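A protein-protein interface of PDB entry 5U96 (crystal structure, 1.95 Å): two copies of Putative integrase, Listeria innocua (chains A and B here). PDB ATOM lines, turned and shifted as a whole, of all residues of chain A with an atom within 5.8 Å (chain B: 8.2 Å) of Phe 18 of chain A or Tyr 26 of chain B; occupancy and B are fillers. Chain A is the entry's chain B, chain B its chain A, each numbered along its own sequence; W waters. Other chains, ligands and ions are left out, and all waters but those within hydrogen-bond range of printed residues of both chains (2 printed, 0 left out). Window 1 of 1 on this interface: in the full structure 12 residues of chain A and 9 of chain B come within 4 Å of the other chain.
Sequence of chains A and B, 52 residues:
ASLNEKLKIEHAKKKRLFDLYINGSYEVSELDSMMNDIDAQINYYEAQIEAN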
ATOM      1  N   LYS A  13      -0.194 -21.521 -31.566  1.00  0.00           N
ATOM      2  CA  LYS A  13      -0.139 -22.954 -31.816  1.00  0.00           C
ATOM      3  C   LYS A  13      -0.245 -23.733 -30.510  1.00  0.00           C
ATOM      4  O   LYS A  13      -0.778 -24.841 -30.477  1.00  0.00           O
ATOM      5  CB  LYS A  13       1.158 -23.317 -32.542  1.00  0.00           C
ATOM      6  CG  LYS A  13       1.170 -22.938 -34.014  1.00  0.00           C
ATOM      7  CD  LYS A  13       2.589 -22.830 -34.557  1.00  0.00           C
ATOM      8  CE  LYS A  13       3.382 -24.105 -34.319  1.00  0.00           C
ATOM      9  NZ  LYS A  13       4.476 -24.273 -35.316  1.00  0.00           N
ATOM     10  N   LYS A  14       0.266 -23.142 -29.434  1.00  0.00           N
ATOM     11  CA  LYS A  14       0.252 -23.782 -28.125  1.00  0.00           C
ATOM     12  C   LYS A  14      -1.167 -23.887 -27.578  1.00  0.00           C
ATOM     13  O   LYS A  14      -1.559 -24.924 -27.042  1.00  0.00           O
ATOM     14  CB  LYS A  14       1.140 -23.007 -27.150  1.00  0.00           C
ATOM     15  CG  LYS A  14       1.316 -23.674 -25.802  1.00  0.00           C
ATOM     16  CD  LYS A  14       2.558 -23.155 -25.097  1.00  0.00           C
ATOM     17  CE  LYS A  14       2.773 -23.840 -23.759  1.00  0.00           C
ATOM     18  NZ  LYS A  14       3.951 -23.286 -23.038  1.00  0.00           N
ATOM     19  N   LYS A  15      -1.933 -22.809 -27.713  1.00  0.00           N
ATOM     20  CA  LYS A  15      -3.322 -22.795 -27.271  1.00  0.00           C
ATOM     21  C   LYS A  15      -4.150 -23.817 -28.038  1.00  0.00           C
ATOM     22  O   LYS A  15      -5.023 -24.474 -27.472  1.00  0.00           O
ATOM     23  CB  LYS A  15      -3.928 -21.401 -27.442  1.00  0.00           C
ATOM     24  CG  LYS A  15      -3.634 -20.452 -26.293  1.00  0.00           C
ATOM     25  CD  LYS A  15      -4.299 -19.100 -26.501  1.00  0.00           C
ATOM     26  CE  LYS A  15      -3.674 -18.034 -25.615  1.00  0.00           C
ATOM     27  NZ  LYS A  15      -4.459 -16.768 -25.609  1.00  0.00           N
ATOM     28  N   ARG A  16      -3.871 -23.947 -29.331  1.00  0.00           N
ATOM     29  CA  ARG A  16      -4.590 -24.887 -30.179  1.00  0.00           C
ATOM     30  C   ARG A  16      -4.189 -26.325 -29.869  1.00  0.00           C
ATOM     31  O   ARG A  16      -5.036 -27.217 -29.823  1.00  0.00           O
ATOM     32  CB  ARG A  16      -4.334 -24.579 -31.655  1.00  0.00           C
ATOM     33  CG  ARG A  16      -4.951 -25.580 -32.624  1.00  0.00           C
ATOM     34  CD  ARG A  16      -6.459 -25.684 -32.447  1.00  0.00           C
ATOM     35  NE  ARG A  16      -7.065 -26.575 -33.432  1.00  0.00           N
ATOM     36  CZ  ARG A  16      -8.364 -26.842 -33.504  1.00  0.00           C
ATOM     37  NH1 ARG A  16      -9.211 -26.288 -32.646  1.00  0.00           N
ATOM     38  NH2 ARG A  16      -8.821 -27.667 -34.436  1.00  0.00           N
ATOM     39  N   LEU A  17      -2.894 -26.545 -29.665  1.00  0.00           N
ATOM     40  CA  LEU A  17      -2.383 -27.879 -29.377  1.00  0.00           C
ATOM     41  C   LEU A  17      -3.019 -28.419 -28.101  1.00  0.00           C
ATOM     42  O   LEU A  17      -3.259 -29.620 -27.975  1.00  0.00           O
ATOM     43  CB  LEU A  17      -0.859 -27.854 -29.252  1.00  0.00           C
ATOM     44  CG  LEU A  17      -0.149 -29.205 -29.149  1.00  0.00           C
ATOM     45  CD1 LEU A  17      -0.568 -30.135 -30.277  1.00  0.00           C
ATOM     46  CD2 LEU A  17       1.357 -29.003 -29.162  1.00  0.00           C
ATOM     47  N   PHE A  18      -3.292 -27.522 -27.162  1.00  0.00           N
ATOM     48  CA  PHE A  18      -4.030 -27.877 -25.958  1.00  0.00           C
ATOM     49  C   PHE A  18      -5.496 -28.146 -26.285  1.00  0.00           C
ATOM     50  O   PHE A  18      -6.110 -29.049 -25.720  1.00  0.00           O
ATOM     51  CB  PHE A  18      -3.932 -26.762 -24.916  1.00  0.00           C
ATOM     52  CG  PHE A  18      -2.673 -26.796 -24.095  1.00  0.00           C
ATOM     53  CD1 PHE A  18      -2.310 -27.937 -23.400  1.00  0.00           C
ATOM     54  CD2 PHE A  18      -1.859 -25.680 -24.012  1.00  0.00           C
ATOM     55  CE1 PHE A  18      -1.156 -27.965 -22.642  1.00  0.00           C
ATOM     56  CE2 PHE A  18      -0.703 -25.703 -23.256  1.00  0.00           C
ATOM     57  CZ  PHE A  18      -0.353 -26.847 -22.569  1.00  0.00           C
ATOM     58  N   ASP A  19      -6.050 -27.349 -27.195  1.00  0.00           N
ATOM     59  CA  ASP A  19      -7.443 -27.491 -27.606  1.00  0.00           C
ATOM     60  C   ASP A  19      -7.693 -28.883 -28.177  1.00  0.00           C
ATOM     61  O   ASP A  19      -8.649 -29.559 -27.798  1.00  0.00           O
ATOM     62  CB  ASP A  19      -7.807 -26.422 -28.643  1.00  0.00           C
ATOM     63  CG  ASP A  19      -9.306 -26.275 -28.838  1.00  0.00           C
ATOM     64  OD1 ASP A  19     -10.065 -27.164 -28.398  1.00  0.00           O
ATOM     65  OD2 ASP A  19      -9.727 -25.268 -29.447  1.00  0.00           O
ATOM     66  N   LEU A  20      -6.823 -29.299 -29.093  1.00  0.00           N
ATOM     67  CA  LEU A  20      -6.933 -30.600 -29.745  1.00  0.00           C
ATOM     68  C   LEU A  20      -6.952 -31.747 -28.743  1.00  0.00           C
ATOM     69  O   LEU A  20      -7.845 -32.595 -28.769  1.00  0.00           O
ATOM     70  CB  LEU A  20      -5.772 -30.799 -30.717  1.00  0.00           C
ATOM     71  CG  LEU A  20      -5.803 -29.936 -31.976  1.00  0.00           C
ATOM     72  CD1 LEU A  20      -4.444 -29.938 -32.655  1.00  0.00           C
ATOM     73  CD2 LEU A  20      -6.879 -30.430 -32.929  1.00  0.00           C
ATOM     74  N   TYR A  21      -5.953 -31.765 -27.869  1.00  0.00           N
ATOM     75  CA  TYR A  21      -5.818 -32.817 -26.870  1.00  0.00           C
ATOM     76  C   TYR A  21      -7.049 -32.897 -25.977  1.00  0.00           C
ATOM     77  O   TYR A  21      -7.547 -33.985 -25.687  1.00  0.00           O
ATOM     78  CB  TYR A  21      -4.569 -32.580 -26.022  1.00  0.00           C
ATOM     79  CG  TYR A  21      -4.578 -33.336 -24.716  1.00  0.00           C
ATOM     80  CD1 TYR A  21      -4.067 -34.621 -24.631  1.00  0.00           C
ATOM     81  CD2 TYR A  21      -5.102 -32.761 -23.567  1.00  0.00           C
ATOM     82  CE1 TYR A  21      -4.080 -35.314 -23.442  1.00  0.00           C
ATOM     83  CE2 TYR A  21      -5.119 -33.442 -22.379  1.00  0.00           C
ATOM     84  CZ  TYR A  21      -4.607 -34.718 -22.317  1.00  0.00           C
ATOM     85  OH  TYR A  21      -4.627 -35.395 -21.124  1.00  0.00           O
ATOM     86  N   ILE A  22      -7.531 -31.738 -25.541  1.00  0.00           N
ATOM     87  CA  ILE A  22      -8.708 -31.667 -24.683  1.00  0.00           C
ATOM     88  C   ILE A  22      -9.915 -32.296 -25.373  1.00  0.00           C
ATOM     89  O   ILE A  22     -10.774 -32.891 -24.720  1.00  0.00           O
ATOM     90  CB  ILE A  22      -9.023 -30.206 -24.294  1.00  0.00           C
ATOM     91  CG1 ILE A  22      -8.036 -29.727 -23.227  1.00  0.00           C
ATOM     92  CG2 ILE A  22     -10.454 -30.079 -23.791  1.00  0.00           C
ATOM     93  CD1 ILE A  22      -8.079 -28.234 -22.966  1.00  0.00           C
ATOM     94  N   ASN A  23      -9.969 -32.169 -26.696  1.00  0.00           N
ATOM     95  CA  ASN A  23     -11.050 -32.752 -27.482  1.00  0.00           C
ATOM     96  C   ASN A  23     -10.733 -34.174 -27.946  1.00  0.00           C
ATOM     97  O   ASN A  23     -11.520 -34.790 -28.663  1.00  0.00           O
ATOM     98  CB  ASN A  23     -11.360 -31.865 -28.688  1.00  0.00           C
ATOM     99  CG  ASN A  23     -11.953 -30.530 -28.289  1.00  0.00           C
ATOM    100  OD1 ASN A  23     -13.159 -30.413 -28.070  1.00  0.00           O
ATOM    101  ND2 ASN A  23     -11.107 -29.512 -28.193  1.00  0.00           N
ATOM    102  N   VAL A  28      -1.975 -38.023 -24.535  1.00  0.00           N
ATOM    103  CA  VAL A  28      -1.017 -37.447 -23.595  1.00  0.00           C
ATOM    104  C   VAL A  28       0.418 -37.720 -24.030  1.00  0.00           C
ATOM    105  O   VAL A  28       1.268 -36.831 -23.991  1.00  0.00           O
ATOM    106  CB  VAL A  28      -1.207 -38.004 -22.169  1.00  0.00           C
ATOM    107  CG1 VAL A  28      -0.163 -37.417 -21.230  1.00  0.00           C
ATOM    108  CG2 VAL A  28      -2.605 -37.711 -21.657  1.00  0.00           C
ATOM    109  N   LEU A  31       1.356 -35.493 -26.794  1.00  0.00           N
ATOM    110  CA  LEU A  31       1.384 -34.106 -26.338  1.00  0.00           C
ATOM    111  C   LEU A  31       2.705 -33.750 -25.660  1.00  0.00           C
ATOM    112  O   LEU A  31       3.136 -32.597 -25.696  1.00  0.00           O
ATOM    113  CB  LEU A  31       0.225 -33.840 -25.376  1.00  0.00           C
ATOM    114  CG  LEU A  31      -0.179 -32.370 -25.249  1.00  0.00           C
ATOM    115  CD1 LEU A  31      -0.857 -31.898 -26.528  1.00  0.00           C
ATOM    116  CD2 LEU A  31      -1.082 -32.151 -24.046  1.00  0.00           C
ATOM    117  N   ASP A  32       3.338 -34.742 -25.043  1.00  0.00           N
ATOM    118  CA  ASP A  32       4.645 -34.558 -24.419  1.00  0.00           C
ATOM    119  C   ASP A  32       5.690 -34.124 -25.441  1.00  0.00           C
ATOM    120  O   ASP A  32       6.411 -33.149 -25.233  1.00  0.00           O
ATOM    121  CB  ASP A  32       5.101 -35.851 -23.738  1.00  0.00           C
ATOM    122  CG  ASP A  32       4.432 -36.076 -22.396  1.00  0.00           C
ATOM    123  OD1 ASP A  32       3.306 -35.574 -22.194  1.00  0.00           O
ATOM    124  OD2 ASP A  32       5.035 -36.757 -21.539  1.00  0.00           O
ATOM    125  N   MET A  35       4.439 -30.633 -27.497  1.00  0.00           N
ATOM    126  CA  MET A  35       4.397 -29.380 -26.752  1.00  0.00           C
ATOM    127  C   MET A  35       5.795 -28.866 -26.429  1.00  0.00           C
ATOM    128  O   MET A  35       6.068 -27.674 -26.567  1.00  0.00           O
ATOM    129  CB  MET A  35       3.599 -29.550 -25.459  1.00  0.00           C
ATOM    130  CG  MET A  35       3.441 -28.258 -24.674  1.00  0.00           C
ATOM    131  SD  MET A  35       2.719 -26.938 -25.663  1.00  0.00           S
ATOM    132  CE  MET A  35       1.052 -27.547 -25.895  1.00  0.00           C
ATOM    133  N   ASP A  39       7.652 -25.254 -27.082  1.00  0.00           N
ATOM    134  CA  ASP A  39       8.316 -24.551 -25.986  1.00  0.00           C
ATOM    135  C   ASP A  39       9.793 -24.316 -26.286  1.00  0.00           C
ATOM    136  O   ASP A  39      10.337 -23.256 -25.976  1.00  0.00           O
ATOM    137  CB  ASP A  39       8.172 -25.339 -24.682  1.00  0.00           C
ATOM    138  CG  ASP A  39       6.730 -25.466 -24.230  1.00  0.00           C
ATOM    139  OD1 ASP A  39       5.917 -24.578 -24.563  1.00  0.00           O
ATOM    140  OD2 ASP A  39       6.410 -26.454 -23.537  1.00  0.00           O
ATOM    141  N   LYS B  13     -13.572 -33.322 -21.532  1.00  0.00           N
ATOM    142  CA  LYS B  13     -12.654 -32.220 -21.794  1.00  0.00           C
ATOM    143  C   LYS B  13     -11.945 -31.808 -20.508  1.00  0.00           C
ATOM    144  O   LYS B  13     -10.815 -31.322 -20.543  1.00  0.00           O
ATOM    145  CB  LYS B  13     -13.395 -31.023 -22.398  1.00  0.00           C
ATOM    146  CG  LYS B  13     -13.763 -31.194 -23.869  1.00  0.00           C
ATOM    147  CD  LYS B  13     -14.535 -29.996 -24.422  1.00  0.00           C
ATOM    148  CE  LYS B  13     -13.750 -28.696 -24.300  1.00  0.00           C
ATOM    149  NZ  LYS B  13     -14.411 -27.568 -25.015  1.00  0.00           N
ATOM    150  N   ARG B  16      -9.276 -35.049 -19.477  1.00  0.00           N
ATOM    151  CA  ARG B  16      -8.079 -35.002 -20.309  1.00  0.00           C
ATOM    152  C   ARG B  16      -7.127 -33.935 -19.792  1.00  0.00           C
ATOM    153  O   ARG B  16      -5.934 -34.174 -19.617  1.00  0.00           O
ATOM    154  CB  ARG B  16      -8.451 -34.716 -21.764  1.00  0.00           C
ATOM    155  CG  ARG B  16      -9.414 -35.725 -22.376  1.00  0.00           C
ATOM    156  CD  ARG B  16      -8.677 -36.846 -23.066  1.00  0.00           C
ATOM    157  NE  ARG B  16      -7.944 -36.370 -24.233  1.00  0.00           N
ATOM    158  CZ  ARG B  16      -6.980 -37.051 -24.839  1.00  0.00           C
ATOM    159  NH1 ARG B  16      -6.614 -38.244 -24.390  1.00  0.00           N
ATOM    160  NH2 ARG B  16      -6.372 -36.534 -25.892  1.00  0.00           N
ATOM    161  N   LEU B  17      -7.684 -32.761 -19.526  1.00  0.00           N
ATOM    162  CA  LEU B  17      -6.923 -31.646 -18.989  1.00  0.00           C
ATOM    163  C   LEU B  17      -6.309 -31.993 -17.638  1.00  0.00           C
ATOM    164  O   LEU B  17      -5.173 -31.615 -17.352  1.00  0.00           O
ATOM    165  CB  LEU B  17      -7.822 -30.416 -18.858  1.00  0.00           C
ATOM    166  CG  LEU B  17      -7.173 -29.122 -18.369  1.00  0.00           C
ATOM    167  CD1 LEU B  17      -6.038 -28.709 -19.293  1.00  0.00           C
ATOM    168  CD2 LEU B  17      -8.217 -28.016 -18.262  1.00  0.00           C
ATOM    169  N   ASP B  19      -5.455 -34.904 -16.624  1.00  0.00           N
ATOM    170  CA  ASP B  19      -4.427 -35.919 -16.825  1.00  0.00           C
ATOM    171  C   ASP B  19      -3.057 -35.281 -17.041  1.00  0.00           C
ATOM    172  O   ASP B  19      -2.028 -35.939 -16.891  1.00  0.00           O
ATOM    173  CB  ASP B  19      -4.776 -36.810 -18.018  1.00  0.00           C
ATOM    174  CG  ASP B  19      -6.172 -37.391 -17.924  1.00  0.00           C
ATOM    175  OD1 ASP B  19      -6.739 -37.400 -16.812  1.00  0.00           O
ATOM    176  OD2 ASP B  19      -6.701 -37.841 -18.961  1.00  0.00           O
ATOM    177  N   LEU B  20      -3.050 -34.001 -17.399  1.00  0.00           N
ATOM    178  CA  LEU B  20      -1.803 -33.270 -17.594  1.00  0.00           C
ATOM    179  C   LEU B  20      -1.240 -32.795 -16.257  1.00  0.00           C
ATOM    180  O   LEU B  20      -0.025 -32.666 -16.100  1.00  0.00           O
ATOM    181  CB  LEU B  20      -2.019 -32.080 -18.532  1.00  0.00           C
ATOM    182  CG  LEU B  20      -2.497 -32.424 -19.946  1.00  0.00           C
ATOM    183  CD1 LEU B  20      -2.670 -31.157 -20.770  1.00  0.00           C
ATOM    184  CD2 LEU B  20      -1.537 -33.384 -20.635  1.00  0.00           C
ATOM    185  N   TYR B  21      -2.123 -32.533 -15.298  1.00  0.00           N
ATOM    186  CA  TYR B  21      -1.694 -32.174 -13.950  1.00  0.00           C
ATOM    187  C   TYR B  21      -1.036 -33.371 -13.266  1.00  0.00           C
ATOM    188  O   TYR B  21       0.011 -33.234 -12.633  1.00  0.00           O
ATOM    189  CB  TYR B  21      -2.871 -31.683 -13.102  1.00  0.00           C
ATOM    190  CG  TYR B  21      -3.452 -30.344 -13.508  1.00  0.00           C
ATOM    191  CD1 TYR B  21      -2.916 -29.154 -13.035  1.00  0.00           C
ATOM    192  CD2 TYR B  21      -4.554 -30.274 -14.342  1.00  0.00           C
ATOM    193  CE1 TYR B  21      -3.458 -27.933 -13.398  1.00  0.00           C
ATOM    194  CE2 TYR B  21      -5.104 -29.063 -14.709  1.00  0.00           C
ATOM    195  CZ  TYR B  21      -4.553 -27.895 -14.235  1.00  0.00           C
ATOM    196  OH  TYR B  21      -5.104 -26.689 -14.604  1.00  0.00           O
ATOM    197  N   ILE B  22      -1.651 -34.543 -13.400  1.00  0.00           N
ATOM    198  CA  ILE B  22      -1.165 -35.741 -12.723  1.00  0.00           C
ATOM    199  C   ILE B  22       0.048 -36.308 -13.455  1.00  0.00           C
ATOM    200  O   ILE B  22       0.888 -36.982 -12.858  1.00  0.00           O
ATOM    201  CB  ILE B  22      -2.269 -36.818 -12.605  1.00  0.00           C
ATOM    202  CG1 ILE B  22      -2.542 -37.496 -13.950  1.00  0.00           C
ATOM    203  CG2 ILE B  22      -3.546 -36.200 -12.072  1.00  0.00           C
ATOM    204  CD1 ILE B  22      -1.974 -38.893 -14.048  1.00  0.00           C
ATOM    205  N   ASN B  23       0.130 -36.028 -14.752  1.00  0.00           N
ATOM    206  CA  ASN B  23       1.339 -36.296 -15.518  1.00  0.00           C
ATOM    207  C   ASN B  23       2.500 -35.519 -14.909  1.00  0.00           C
ATOM    208  O   ASN B  23       3.641 -35.985 -14.903  1.00  0.00           O
ATOM    209  CB  ASN B  23       1.135 -35.920 -16.987  1.00  0.00           C
ATOM    210  CG  ASN B  23       2.439 -35.818 -17.755  1.00  0.00           C
ATOM    211  OD1 ASN B  23       3.195 -34.860 -17.596  1.00  0.00           O
ATOM    212  ND2 ASN B  23       2.696 -36.797 -18.613  1.00  0.00           N
ATOM    213  N   GLY B  24       2.194 -34.326 -14.405  1.00  0.00           N
ATOM    214  CA  GLY B  24       3.124 -33.567 -13.590  1.00  0.00           C
ATOM    215  C   GLY B  24       3.892 -32.504 -14.351  1.00  0.00           C
ATOM    216  O   GLY B  24       4.282 -31.491 -13.774  1.00  0.00           O
ATOM    217  N   SER B  25       4.113 -32.726 -15.642  1.00  0.00           N
ATOM    218  CA  SER B  25       4.836 -31.757 -16.459  1.00  0.00           C
ATOM    219  C   SER B  25       3.942 -30.560 -16.780  1.00  0.00           C
ATOM    220  O   SER B  25       2.882 -30.398 -16.178  1.00  0.00           O
ATOM    221  CB  SER B  25       5.355 -32.420 -17.739  1.00  0.00           C
ATOM    222  OG  SER B  25       6.524 -33.175 -17.471  1.00  0.00           O
ATOM    223  N   TYR B  26       4.391 -29.720 -17.711  1.00  0.00           N
ATOM    224  CA  TYR B  26       3.679 -28.505 -18.110  1.00  0.00           C
ATOM    225  C   TYR B  26       3.631 -27.474 -16.986  1.00  0.00           C
ATOM    226  O   TYR B  26       3.927 -27.778 -15.831  1.00  0.00           O
ATOM    227  CB  TYR B  26       2.249 -28.823 -18.562  1.00  0.00           C
ATOM    228  CG  TYR B  26       2.157 -29.808 -19.701  1.00  0.00           C
ATOM    229  CD1 TYR B  26       2.194 -29.377 -21.017  1.00  0.00           C
ATOM    230  CD2 TYR B  26       2.022 -31.169 -19.462  1.00  0.00           C
ATOM    231  CE1 TYR B  26       2.107 -30.270 -22.063  1.00  0.00           C
ATOM    232  CE2 TYR B  26       1.934 -32.071 -20.505  1.00  0.00           C
ATOM    233  CZ  TYR B  26       1.977 -31.614 -21.804  1.00  0.00           C
ATOM    234  OH  TYR B  26       1.889 -32.503 -22.850  1.00  0.00           O
ATOM    235  N   GLU B  27       3.256 -26.249 -17.344  1.00  0.00           N
ATOM    236  CA  GLU B  27       3.065 -25.186 -16.367  1.00  0.00           C
ATOM    237  C   GLU B  27       1.592 -25.116 -15.984  1.00  0.00           C
ATOM    238  O   GLU B  27       0.713 -25.161 -16.845  1.00  0.00           O
ATOM    239  CB  GLU B  27       3.541 -23.841 -16.917  1.00  0.00           C
ATOM    240  CG  GLU B  27       3.533 -22.722 -15.887  1.00  0.00           C
ATOM    241  CD  GLU B  27       3.932 -21.383 -16.472  1.00  0.00           C
ATOM    242  OE1 GLU B  27       4.220 -21.322 -17.686  1.00  0.00           O
ATOM    243  OE2 GLU B  27       3.955 -20.388 -15.716  1.00  0.00           O
ATOM    244  N   VAL B  28       1.330 -25.003 -14.689  1.00  0.00           N
ATOM    245  CA  VAL B  28      -0.028 -25.085 -14.171  1.00  0.00           C
ATOM    246  C   VAL B  28      -0.859 -23.872 -14.580  1.00  0.00           C
ATOM    247  O   VAL B  28      -2.077 -23.969 -14.724  1.00  0.00           O
ATOM    248  CB  VAL B  28      -0.026 -25.205 -12.634  1.00  0.00           C
ATOM    249  CG1 VAL B  28       0.860 -26.374 -12.188  1.00  0.00           C
ATOM    250  CG2 VAL B  28       0.432 -23.899 -12.003  1.00  0.00           C
ATOM    251  N   SER B  29      -0.199 -22.732 -14.767  1.00  0.00           N
ATOM    252  CA  SER B  29      -0.890 -21.503 -15.143  1.00  0.00           C
ATOM    253  C   SER B  29      -1.456 -21.610 -16.555  1.00  0.00           C
ATOM    254  O   SER B  29      -2.508 -21.046 -16.854  1.00  0.00           O
ATOM    255  CB  SER B  29       0.054 -20.303 -15.041  1.00  0.00           C
ATOM    256  OG  SER B  29       1.122 -20.415 -15.964  1.00  0.00           O
ATOM    257  N   GLU B  30      -0.750 -22.330 -17.421  1.00  0.00           N
ATOM    258  CA  GLU B  30      -1.248 -22.614 -18.761  1.00  0.00           C
ATOM    259  C   GLU B  30      -2.535 -23.425 -18.676  1.00  0.00           C
ATOM    260  O   GLU B  30      -3.510 -23.144 -19.374  1.00  0.00           O
ATOM    261  CB  GLU B  30      -0.204 -23.378 -19.581  1.00  0.00           C
ATOM    262  CG  GLU B  30       1.129 -22.662 -19.743  1.00  0.00           C
ATOM    263  CD  GLU B  30       2.163 -23.516 -20.454  1.00  0.00           C
ATOM    264  OE1 GLU B  30       1.840 -24.668 -20.817  1.00  0.00           O
ATOM    265  OE2 GLU B  30       3.300 -23.038 -20.650  1.00  0.00           O
ATOM    266  N   LEU B  31      -2.527 -24.430 -17.807  1.00  0.00           N
ATOM    267  CA  LEU B  31      -3.649 -25.349 -17.667  1.00  0.00           C
ATOM    268  C   LEU B  31      -4.824 -24.709 -16.926  1.00  0.00           C
ATOM    269  O   LEU B  31      -5.958 -25.179 -17.029  1.00  0.00           O
ATOM    270  CB  LEU B  31      -3.197 -26.615 -16.932  1.00  0.00           C
ATOM    271  CG  LEU B  31      -1.995 -27.369 -17.505  1.00  0.00           C
ATOM    272  CD1 LEU B  31      -1.479 -28.366 -16.480  1.00  0.00           C
ATOM    273  CD2 LEU B  31      -2.360 -28.077 -18.800  1.00  0.00           C
ATOM    274  N   MET B  34      -7.513 -22.495 -19.415  1.00  0.00           N
ATOM    275  CA  MET B  34      -8.521 -23.244 -20.157  1.00  0.00           C
ATOM    276  C   MET B  34      -9.507 -23.909 -19.209  1.00  0.00           C
ATOM    277  O   MET B  34     -10.666 -24.122 -19.556  1.00  0.00           O
ATOM    278  CB  MET B  34      -7.863 -24.292 -21.046  1.00  0.00           C
ATOM    279  CG  MET B  34      -6.820 -23.718 -21.982  1.00  0.00           C
ATOM    280  SD  MET B  34      -5.983 -24.982 -22.942  1.00  0.00           S
ATOM    281  CE  MET B  34      -5.046 -25.813 -21.663  1.00  0.00           C
ATOM    282  N   ILE B  38     -13.359 -24.114 -19.201  1.00  0.00           N
ATOM    283  CA  ILE B  38     -14.023 -25.410 -19.121  1.00  0.00           C
ATOM    284  C   ILE B  38     -14.986 -25.469 -17.934  1.00  0.00           C
ATOM    285  O   ILE B  38     -16.113 -25.938 -18.074  1.00  0.00           O
ATOM    286  CB  ILE B  38     -12.998 -26.561 -19.016  1.00  0.00           C
ATOM    287  CG1 ILE B  38     -12.342 -26.800 -20.381  1.00  0.00           C
ATOM    288  CG2 ILE B  38     -13.674 -27.834 -18.521  1.00  0.00           C
ATOM    289  CD1 ILE B  38     -11.235 -27.835 -20.368  1.00  0.00           C
HETATM  290  O   HOH W   1      -5.851 -38.051 -21.375  1.00  0.00           O
HETATM  291  O   HOH W   2       4.743 -33.826 -20.419  1.00  0.00           O
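The side-chain hydroxyl of Tyr 26 of chain B lies within hydrogen-bond range of the side-chain carboxylate of Asp 32 of chain A (3.4 Å). The side-chain hydroxyl (OH) of Tyr 26 of chain B is in hydrogen-bond range of the backbone carbonyl oxygen (O) of Leu 31 of chain A, at 3.1 Å. The guanidinium group (NH2) of Arg 16 of chain B is in hydrogen-bond range of the backbone carbonyl oxygen (O) of Tyr 21 of chain A, at 2.8 Å. NZ of Lys 14 of chain A lies within salt-bridge range of OE2 of Glu 30 of chain B (2.5 Å).
OD1 of Asn 23 of chain B lies within hydrogen-bond range of N of Ser 25 of chain B (3.0 Å). The side-chain amino group (NZ) of Lys 14 of chain A is in salt-bridge range of the side-chain carboxylate (OD1) of Asp 39 of chain A (2.8 Å). The side-chain amide nitrogen of Asn 23 of chain A lies within hydrogen-bond range of the backbone carbonyl oxygen of Asp 19 of chain A (2.5 Å).
Among the printed residues, merely in contact across the chains: Phe 18 of chain A with Leu 20 of chain B, Phe 18 of chain A with Tyr 26 of chain B, Phe 18 of chain A with Glu 30 of chain B, Phe 18 of chain A with Met 34 of chain B, Tyr 21 of chain A with Leu 17 of chain B, Tyr 21 of chain A with Asp 19 of chain B, Tyr 21 of chain A with Leu 20 of chain B, Ile 22 of chain A with Lys 13 of chain B, Ile 22 of chain A with Arg 16 of chain B, Ile 22 of chain A with Met 34 of chain B, Asn 23 of chain A with Lys 13 of chain B, Val 28 of chain A with Asn 23 of chain B, Leu 31 of chain A with Leu 20 of chain B, Asp 32 of chain A with Asn 23 of chain B and Met 35 of chain A with Tyr 26 of chain B.
Printed residues of chain B within 4 Å of Phe 18 of chain A: Leu 20, Tyr 26, Glu 30 and Met 34. Printed residues of chain A within 4 Å of Asp 19 of chain B: Tyr 21. Of chain A, only Phe 18, Leu 31, Asp 32 and Met 35 come within 4 Å of Tyr 26 of chain B. Of the printed residues of chain A, Met 34 of chain B touches Phe 18 (3.4 Å) and Ile 22 (3.9 Å).
Hydrophobic or aromatic side chains of chain B within 4 Å of the printed part of chain A: Leu 20, Tyr 26 and Met 34. Of the 16 printed residues of chain A, 9 touch a printed residue of chain B. Hydrophobic or aromatic side chains of chain A within 4 Å of the printed part of chain B: Phe 18, Tyr 21, Ile 22, Val 28, Leu 31 and Met 35.
Tyr 21 of chain A touches Leu 17 of chain B, but with the chains exchanged Leu 17 of chain A does not touch Tyr 21 of chain B (13.1 Å). Tyr 21 of chain A touches Leu 20 of chain B, but with the chains exchanged Leu 20 of chain A does not touch Tyr 21 of chain B (14.3 Å). Ile 22 of chain A touches Arg 16 of chain B, but with the chains exchanged Arg 16 of chain A does not touch Ile 22 of chain B (18.3 Å). Asn 23 of chain A touches Lys 13 of chain B, but with the chains exchanged Lys 13 of chain A does not touch Asn 23 of chain B (16.8 Å).
Water W1 lies within hydrogen-bond range of the side-chain carboxylate of Asp 19 of chain B (2.6 Å), the side-chain hydroxyl of Tyr 21 of chain A (2.9 Å) and the guanidinium group of Arg 16 of chain B (3.1 Å). Water W2 bridges the side-chain carboxylate (OD1) of Asp 32 of chain A (2.9 Å) and the side-chain amide oxygen (OD1) of Asn 23 of chain B (3.4 Å).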
